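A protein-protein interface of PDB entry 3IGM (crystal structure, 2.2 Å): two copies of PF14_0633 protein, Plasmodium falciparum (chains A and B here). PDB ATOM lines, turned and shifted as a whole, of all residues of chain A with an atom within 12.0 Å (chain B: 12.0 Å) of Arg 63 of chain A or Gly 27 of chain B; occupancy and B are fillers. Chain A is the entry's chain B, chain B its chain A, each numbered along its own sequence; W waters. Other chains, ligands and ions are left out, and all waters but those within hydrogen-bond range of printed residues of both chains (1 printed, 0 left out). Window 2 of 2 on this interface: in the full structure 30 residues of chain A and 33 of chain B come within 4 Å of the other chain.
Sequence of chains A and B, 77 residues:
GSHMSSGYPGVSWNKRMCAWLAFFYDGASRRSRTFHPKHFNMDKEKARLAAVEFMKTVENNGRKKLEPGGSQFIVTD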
ATOM      1  N   PHE A  54     -22.237  14.224  25.447  1.00  0.00           N
ATOM      2  CA  PHE A  54     -20.904  13.668  25.227  1.00  0.00           C
ATOM      3  C   PHE A  54     -20.687  13.284  23.763  1.00  0.00           C
ATOM      4  O   PHE A  54     -19.600  13.489  23.216  1.00  0.00           O
ATOM      5  CB  PHE A  54     -20.596  12.461  26.124  1.00  0.00           C
ATOM      6  CG  PHE A  54     -19.335  11.735  25.718  1.00  0.00           C
ATOM      7  CD1 PHE A  54     -18.081  12.272  26.015  1.00  0.00           C
ATOM      8  CD2 PHE A  54     -19.400  10.551  24.981  1.00  0.00           C
ATOM      9  CE1 PHE A  54     -16.913  11.628  25.608  1.00  0.00           C
ATOM     10  CE2 PHE A  54     -18.246   9.900  24.574  1.00  0.00           C
ATOM     11  CZ  PHE A  54     -16.997  10.436  24.888  1.00  0.00           C
ATOM     12  N   MET A  55     -21.721  12.701  23.156  1.00  0.00           N
ATOM     13  CA  MET A  55     -21.672  12.280  21.757  1.00  0.00           C
ATOM     14  C   MET A  55     -21.317  13.446  20.832  1.00  0.00           C
ATOM     15  O   MET A  55     -20.536  13.279  19.894  1.00  0.00           O
ATOM     16  CB  MET A  55     -23.002  11.635  21.337  1.00  0.00           C
ATOM     17  CG  MET A  55     -23.006  11.070  19.925  1.00  0.00           C
ATOM     18  SD  MET A  55     -21.692   9.865  19.634  1.00  0.00           S
ATOM     19  CE  MET A  55     -22.427   8.456  20.371  1.00  0.00           C
ATOM     20  N   LYS A  56     -21.885  14.617  21.120  1.00  0.00           N
ATOM     21  CA  LYS A  56     -21.662  15.835  20.334  1.00  0.00           C
ATOM     22  C   LYS A  56     -20.219  16.335  20.420  1.00  0.00           C
ATOM     23  O   LYS A  56     -19.681  16.877  19.444  1.00  0.00           O
ATOM     24  CB  LYS A  56     -22.627  16.934  20.775  1.00  0.00           C
ATOM     25  CG  LYS A  56     -24.076  16.660  20.411  1.00  0.00           C
ATOM     26  CD  LYS A  56     -24.959  17.869  20.674  1.00  0.00           C
ATOM     27  CE  LYS A  56     -26.384  17.620  20.194  1.00  0.00           C
ATOM     28  NZ  LYS A  56     -26.447  17.429  18.712  1.00  0.00           N
ATOM     29  N   THR A  57     -19.615  16.141  21.595  1.00  0.00           N
ATOM     30  CA  THR A  57     -18.208  16.435  21.867  1.00  0.00           C
ATOM     31  C   THR A  57     -17.277  15.637  20.959  1.00  0.00           C
ATOM     32  O   THR A  57     -16.171  16.082  20.626  1.00  0.00           O
ATOM     33  CB  THR A  57     -17.880  16.103  23.346  1.00  0.00           C
ATOM     34  OG1 THR A  57     -18.409  17.129  24.192  1.00  0.00           O
ATOM     35  CG2 THR A  57     -16.378  15.970  23.587  1.00  0.00           C
ATOM     36  N   VAL A  58     -17.745  14.463  20.547  1.00  0.00           N
ATOM     37  CA  VAL A  58     -16.908  13.510  19.838  1.00  0.00           C
ATOM     38  C   VAL A  58     -17.358  13.296  18.368  1.00  0.00           C
ATOM     39  O   VAL A  58     -17.015  12.295  17.723  1.00  0.00           O
ATOM     40  CB  VAL A  58     -16.790  12.210  20.681  1.00  0.00           C
ATOM     41  CG1 VAL A  58     -18.009  11.302  20.521  1.00  0.00           C
ATOM     42  CG2 VAL A  58     -15.505  11.501  20.381  1.00  0.00           C
ATOM     43  N   GLU A  59     -18.102  14.266  17.842  1.00  0.00           N
ATOM     44  CA  GLU A  59     -18.557  14.232  16.446  1.00  0.00           C
ATOM     45  C   GLU A  59     -17.612  14.985  15.516  1.00  0.00           C
ATOM     46  O   GLU A  59     -17.963  16.027  14.949  1.00  0.00           O
ATOM     47  CB  GLU A  59     -19.981  14.773  16.326  1.00  0.00           C
ATOM     48  CG  GLU A  59     -21.037  13.761  16.703  1.00  0.00           C
ATOM     49  CD  GLU A  59     -22.416  14.368  16.854  1.00  0.00           C
ATOM     50  OE1 GLU A  59     -22.577  15.600  16.701  1.00  0.00           O
ATOM     51  OE2 GLU A  59     -23.353  13.597  17.130  1.00  0.00           O
ATOM     52  N   ASN A  60     -16.401  14.446  15.387  1.00  0.00           N
ATOM     53  CA  ASN A  60     -15.355  15.004  14.531  1.00  0.00           C
ATOM     54  C   ASN A  60     -14.440  13.892  14.030  1.00  0.00           C
ATOM     55  O   ASN A  60     -14.555  12.743  14.461  1.00  0.00           O
ATOM     56  CB  ASN A  60     -14.572  16.103  15.266  1.00  0.00           C
ATOM     57  CG  ASN A  60     -13.845  15.583  16.496  1.00  0.00           C
ATOM     58  OD1 ASN A  60     -12.734  15.057  16.397  1.00  0.00           O
ATOM     59  ND2 ASN A  60     -14.466  15.736  17.664  1.00  0.00           N
ATOM     60  N   ASN A  61     -13.540  14.225  13.111  1.00  0.00           N
ATOM     61  CA  ASN A  61     -12.621  13.226  12.554  1.00  0.00           C
ATOM     62  C   ASN A  61     -11.177  13.254  13.093  1.00  0.00           C
ATOM     63  O   ASN A  61     -10.352  12.408  12.727  1.00  0.00           O
ATOM     64  CB  ASN A  61     -12.661  13.216  11.015  1.00  0.00           C
ATOM     65  CG  ASN A  61     -12.406  14.587  10.381  1.00  0.00           C
ATOM     66  OD1 ASN A  61     -12.528  14.729   9.163  1.00  0.00           O
ATOM     67  ND2 ASN A  61     -12.048  15.586  11.187  1.00  0.00           N
ATOM     68  N   GLY A  62     -10.893  14.215  13.970  1.00  0.00           N
ATOM     69  CA  GLY A  62      -9.600  14.293  14.646  1.00  0.00           C
ATOM     70  C   GLY A  62      -9.457  13.235  15.728  1.00  0.00           C
ATOM     71  O   GLY A  62     -10.436  12.577  16.109  1.00  0.00           O
ATOM     72  N   ARG A  63      -8.232  13.068  16.219  1.00  0.00           N
ATOM     73  CA  ARG A  63      -7.961  12.151  17.331  1.00  0.00           C
ATOM     74  C   ARG A  63      -8.546  12.658  18.658  1.00  0.00           C
ATOM     75  O   ARG A  63      -8.695  13.867  18.862  1.00  0.00           O
ATOM     76  CB  ARG A  63      -6.461  11.885  17.451  1.00  0.00           C
ATOM     77  CG  ARG A  63      -5.896  11.029  16.314  1.00  0.00           C
ATOM     78  CD  ARG A  63      -6.349   9.565  16.407  1.00  0.00           C
ATOM     79  NE  ARG A  63      -5.931   8.949  17.664  1.00  0.00           N
ATOM     80  CZ  ARG A  63      -5.992   7.648  17.932  1.00  0.00           C
ATOM     81  NH1 ARG A  63      -6.455   6.788  17.030  1.00  0.00           N
ATOM     82  NH2 ARG A  63      -5.582   7.205  19.113  1.00  0.00           N
ATOM     83  N   LYS A  64      -8.874  11.726  19.549  1.00  0.00           N
ATOM     84  CA  LYS A  64      -9.620  12.035  20.776  1.00  0.00           C
ATOM     85  C   LYS A  64      -8.748  12.142  22.030  1.00  0.00           C
ATOM     86  O   LYS A  64      -7.550  11.852  21.988  1.00  0.00           O
ATOM     87  CB  LYS A  64     -10.730  10.992  20.990  1.00  0.00           C
ATOM     88  CG  LYS A  64     -12.073  11.365  20.372  1.00  0.00           C
ATOM     89  CD  LYS A  64     -12.030  11.430  18.852  1.00  0.00           C
ATOM     90  CE  LYS A  64     -13.080  12.382  18.308  1.00  0.00           C
ATOM     91  NZ  LYS A  64     -13.191  12.299  16.830  1.00  0.00           N
ATOM     92  N   LYS A  65      -9.365  12.565  23.135  1.00  0.00           N
ATOM     93  CA  LYS A  65      -8.707  12.600  24.449  1.00  0.00           C
ATOM     94  C   LYS A  65      -8.620  11.212  25.086  1.00  0.00           C
ATOM     95  O   LYS A  65      -8.367  10.212  24.403  1.00  0.00           O
ATOM     96  CB  LYS A  65      -9.441  13.543  25.402  1.00  0.00           C
ATOM     97  CG  LYS A  65      -9.181  15.023  25.155  1.00  0.00           C
ATOM     98  CD  LYS A  65      -9.370  15.854  26.441  1.00  0.00           C
ATOM     99  CE  LYS A  65     -10.827  15.899  26.923  1.00  0.00           C
ATOM    100  NZ  LYS A  65     -11.729  16.641  25.986  1.00  0.00           N
ATOM    101  N   PHE B  23     -21.287   5.549  21.186  1.00  0.00           N
ATOM    102  CA  PHE B  23     -20.267   4.953  20.325  1.00  0.00           C
ATOM    103  C   PHE B  23     -19.622   5.998  19.425  1.00  0.00           C
ATOM    104  O   PHE B  23     -20.309   6.755  18.739  1.00  0.00           O
ATOM    105  CB  PHE B  23     -20.839   3.780  19.524  1.00  0.00           C
ATOM    106  CG  PHE B  23     -20.981   2.510  20.331  1.00  0.00           C
ATOM    107  CD1 PHE B  23     -20.039   1.486  20.214  1.00  0.00           C
ATOM    108  CD2 PHE B  23     -22.047   2.343  21.219  1.00  0.00           C
ATOM    109  CE1 PHE B  23     -20.161   0.308  20.969  1.00  0.00           C
ATOM    110  CE2 PHE B  23     -22.177   1.168  21.971  1.00  0.00           C
ATOM    111  CZ  PHE B  23     -21.237   0.152  21.847  1.00  0.00           C
ATOM    112  N   PHE B  24     -18.294   6.038  19.444  1.00  0.00           N
ATOM    113  CA  PHE B  24     -17.556   7.044  18.699  1.00  0.00           C
ATOM    114  C   PHE B  24     -16.275   6.517  18.069  1.00  0.00           C
ATOM    115  O   PHE B  24     -15.904   5.360  18.265  1.00  0.00           O
ATOM    116  CB  PHE B  24     -17.275   8.281  19.571  1.00  0.00           C
ATOM    117  CG  PHE B  24     -16.453   8.007  20.818  1.00  0.00           C
ATOM    118  CD1 PHE B  24     -15.094   8.334  20.860  1.00  0.00           C
ATOM    119  CD2 PHE B  24     -17.039   7.465  21.958  1.00  0.00           C
ATOM    120  CE1 PHE B  24     -14.327   8.115  22.015  1.00  0.00           C
ATOM    121  CE2 PHE B  24     -16.279   7.230  23.112  1.00  0.00           C
ATOM    122  CZ  PHE B  24     -14.922   7.561  23.141  1.00  0.00           C
ATOM    123  N   TYR B  25     -15.622   7.379  17.294  1.00  0.00           N
ATOM    124  CA  TYR B  25     -14.380   7.032  16.628  1.00  0.00           C
ATOM    125  C   TYR B  25     -13.242   7.913  17.099  1.00  0.00           C
ATOM    126  O   TYR B  25     -13.317   9.142  17.032  1.00  0.00           O
ATOM    127  CB  TYR B  25     -14.533   7.104  15.102  1.00  0.00           C
ATOM    128  CG  TYR B  25     -15.406   6.001  14.566  1.00  0.00           C
ATOM    129  CD1 TYR B  25     -14.862   4.773  14.188  1.00  0.00           C
ATOM    130  CD2 TYR B  25     -16.789   6.174  14.471  1.00  0.00           C
ATOM    131  CE1 TYR B  25     -15.678   3.751  13.711  1.00  0.00           C
ATOM    132  CE2 TYR B  25     -17.606   5.169  13.998  1.00  0.00           C
ATOM    133  CZ  TYR B  25     -17.053   3.962  13.620  1.00  0.00           C
ATOM    134  OH  TYR B  25     -17.888   2.971  13.157  1.00  0.00           O
ATOM    135  N   ASP B  26     -12.205   7.253  17.606  1.00  0.00           N
ATOM    136  CA  ASP B  26     -10.953   7.884  17.962  1.00  0.00           C
ATOM    137  C   ASP B  26     -10.012   7.522  16.824  1.00  0.00           C
ATOM    138  O   ASP B  26      -9.251   6.553  16.908  1.00  0.00           O
ATOM    139  CB  ASP B  26     -10.462   7.335  19.308  1.00  0.00           C
ATOM    140  CG  ASP B  26      -9.180   8.001  19.798  1.00  0.00           C
ATOM    141  OD1 ASP B  26      -8.659   7.565  20.856  1.00  0.00           O
ATOM    142  OD2 ASP B  26      -8.687   8.951  19.143  1.00  0.00           O
ATOM    143  N   GLY B  27     -10.094   8.300  15.747  1.00  0.00           N
ATOM    144  CA  GLY B  27      -9.390   8.000  14.502  1.00  0.00           C
ATOM    145  C   GLY B  27      -9.839   6.676  13.909  1.00  0.00           C
ATOM    146  O   GLY B  27     -10.989   6.535  13.475  1.00  0.00           O
ATOM    147  N   ALA B  28      -8.922   5.707  13.913  1.00  0.00           N
ATOM    148  CA  ALA B  28      -9.161   4.358  13.385  1.00  0.00           C
ATOM    149  C   ALA B  28      -9.992   3.493  14.328  1.00  0.00           C
ATOM    150  O   ALA B  28     -10.789   2.664  13.879  1.00  0.00           O
ATOM    151  CB  ALA B  28      -7.829   3.666  13.078  1.00  0.00           C
ATOM    152  N   SER B  29      -9.797   3.678  15.628  1.00  0.00           N
ATOM    153  CA  SER B  29     -10.457   2.832  16.616  1.00  0.00           C
ATOM    154  C   SER B  29     -11.884   3.273  16.928  1.00  0.00           C
ATOM    155  O   SER B  29     -12.172   4.467  17.046  1.00  0.00           O
ATOM    156  CB  SER B  29      -9.625   2.701  17.900  1.00  0.00           C
ATOM    157  OG  SER B  29      -8.849   3.861  18.148  1.00  0.00           O
ATOM    158  N   ARG B  30     -12.766   2.284  17.048  1.00  0.00           N
ATOM    159  CA  ARG B  30     -14.123   2.502  17.522  1.00  0.00           C
ATOM    160  C   ARG B  30     -14.151   2.386  19.045  1.00  0.00           C
ATOM    161  O   ARG B  30     -13.654   1.411  19.624  1.00  0.00           O
ATOM    162  CB  ARG B  30     -15.092   1.509  16.883  1.00  0.00           C
ATOM    163  CG  ARG B  30     -16.543   1.921  17.029  1.00  0.00           C
ATOM    164  CD  ARG B  30     -17.479   1.065  16.207  1.00  0.00           C
ATOM    165  NE  ARG B  30     -18.826   1.627  16.246  1.00  0.00           N
ATOM    166  CZ  ARG B  30     -19.946   0.939  16.037  1.00  0.00           C
ATOM    167  NH1 ARG B  30     -19.901  -0.367  15.770  1.00  0.00           N
ATOM    168  NH2 ARG B  30     -21.119   1.564  16.099  1.00  0.00           N
ATOM    169  N   ARG B  31     -14.727   3.396  19.684  1.00  0.00           N
ATOM    170  CA  ARG B  31     -14.738   3.485  21.139  1.00  0.00           C
ATOM    171  C   ARG B  31     -16.165   3.602  21.647  1.00  0.00           C
ATOM    172  O   ARG B  31     -17.083   3.839  20.857  1.00  0.00           O
ATOM    173  CB  ARG B  31     -13.907   4.691  21.594  1.00  0.00           C
ATOM    174  CG  ARG B  31     -12.483   4.732  21.046  1.00  0.00           C
ATOM    175  CD  ARG B  31     -11.463   4.218  22.036  1.00  0.00           C
ATOM    176  NE  ARG B  31     -11.024   5.281  22.938  1.00  0.00           N
ATOM    177  CZ  ARG B  31     -11.524   5.510  24.154  1.00  0.00           C
ATOM    178  NH1 ARG B  31     -12.496   4.749  24.650  1.00  0.00           N
ATOM    179  NH2 ARG B  31     -11.048   6.513  24.884  1.00  0.00           N
ATOM    180  N   SER B  32     -16.353   3.406  22.953  1.00  0.00           N
ATOM    181  CA  SER B  32     -17.643   3.658  23.601  1.00  0.00           C
ATOM    182  C   SER B  32     -17.494   4.164  25.038  1.00  0.00           C
ATOM    183  O   SER B  32     -16.571   3.763  25.759  1.00  0.00           O
ATOM    184  CB  SER B  32     -18.561   2.426  23.546  1.00  0.00           C
ATOM    185  OG  SER B  32     -18.297   1.503  24.596  1.00  0.00           O
ATOM    186  N   ARG B  33     -18.398   5.065  25.428  1.00  0.00           N
ATOM    187  CA  ARG B  33     -18.534   5.506  26.823  1.00  0.00           C
ATOM    188  C   ARG B  33     -19.930   5.203  27.364  1.00  0.00           C
ATOM    189  O   ARG B  33     -20.935   5.426  26.689  1.00  0.00           O
ATOM    190  CB  ARG B  33     -18.191   6.997  27.011  1.00  0.00           C
ATOM    191  CG  ARG B  33     -18.309   7.459  28.483  1.00  0.00           C
ATOM    192  CD  ARG B  33     -17.598   8.761  28.788  1.00  0.00           C
ATOM    193  NE  ARG B  33     -16.236   8.757  28.262  1.00  0.00           N
ATOM    194  CZ  ARG B  33     -15.299   9.641  28.579  1.00  0.00           C
ATOM    195  NH1 ARG B  33     -15.553  10.616  29.447  1.00  0.00           N
ATOM    196  NH2 ARG B  33     -14.097   9.541  28.029  1.00  0.00           N
HETATM  197  O   HOH W   1      -5.690   5.721  14.692  1.00  0.00           O
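No position is printed for both chains.
Of the 9 pairs that touch across the chains among the printed residues, none has its exchanged pair printed and touching as well.
Of the printed residues of chain B, Met 55 of chain A touches Phe 23.
Printed residues of chain B within 4 Å of Val 58 of chain A: Phe 24.
No residue of chain B comes within 4 Å of Gly 62 of chain A.
Arg 63 of chain A touches three residues of chain B.
Printed residues of chain A within 4 Å of Phe 24 of chain B: Phe 54 and Val 58.
Of chain A, only Arg 63 (3.9 Å) comes within 4 Å of Gly 27 of chain B.
Ser 29 of chain B touches just one residue of chain A: Arg 63 (3.9 Å).
The nearest residue of chain B that does not touch Arg 63 of chain A is Ala 28 of chain B (4.1 Å).
The nearest printed residue of chain B that does not touch Val 58 of chain A is Tyr 25 of chain B (4.6 Å).
Hydrophobic or aromatic side chains of chain A within 4 Å of the printed part of chain B: Phe 54, Met 55 and Val 58.
Of the 11 printed residues of chain B, 7 touch a printed residue of chain A.
Hydrophobic or aromatic side chains of chain B within 4 Å of the printed part of chain A: Phe 24.
Along chain B the printed residues that touch a printed residue of chain A span positions 23 to 33.
O of Asn 60 of chain A sits at hydrogen-bond distance from NZ of Lys 64 of chain A (2.8 Å).
The backbone carbonyl oxygen (O) of Gly 62 of chain A is in hydrogen-bond range of the side-chain amino group (NZ) of Lys 64 of chain A, 2.9 Å away.
O of Phe 24 of chain B sits at hydrogen-bond distance from N of Arg 31 of chain B (2.7 Å).
The side-chain hydroxyl (OH) of Tyr 25 of chain B lies within hydrogen-bond range of the guanidinium group (NE) of Arg 30 of chain B.
O of Asp 26 of chain B is in hydrogen-bond range of OG of Ser 29 of chain B (3.0 Å).
The side-chain carboxylate (OD1) of Asp 26 of chain B is in salt-bridge range of the guanidinium group (NE) of Arg 31 of chain B.
Water W1 bridges the guanidinium group of Arg 63 of chain A (2.7 Å) and the backbone NH of Ala 28 of chain B (3.3 Å).
The side-chain carboxylate (OD2) of Asp 26 of chain B is in salt-bridge range of the guanidinium group (NE) of Arg 63 of chain A (3.1 Å).
The side-chain amino group (NZ) of Lys 64 of chain A lies within hydrogen-bond range of the backbone carbonyl oxygen (O) of Tyr 25 of chain B.
The backbone NH (N) of Lys 64 of chain A sits at hydrogen-bond distance from the side-chain carboxylate (OD2) of Asp 26 of chain B.
O of Phe 23 of chain B lies close to SD of Met 55 of chain A (3.5 Å).
Among the printed residues, merely in contact across the chains: Val 58 of chain A with Phe 24 of chain B (3.2 Å), Phe 54 of chain A with Phe 24 of chain B (3.6 Å), Phe 54 of chain A with Arg 33 of chain B (3.8 Å), Arg 63 of chain A with Gly 27 of chain B (3.9 Å) and Arg 63 of chain A with Ser 29 of chain B (3.9 Å).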
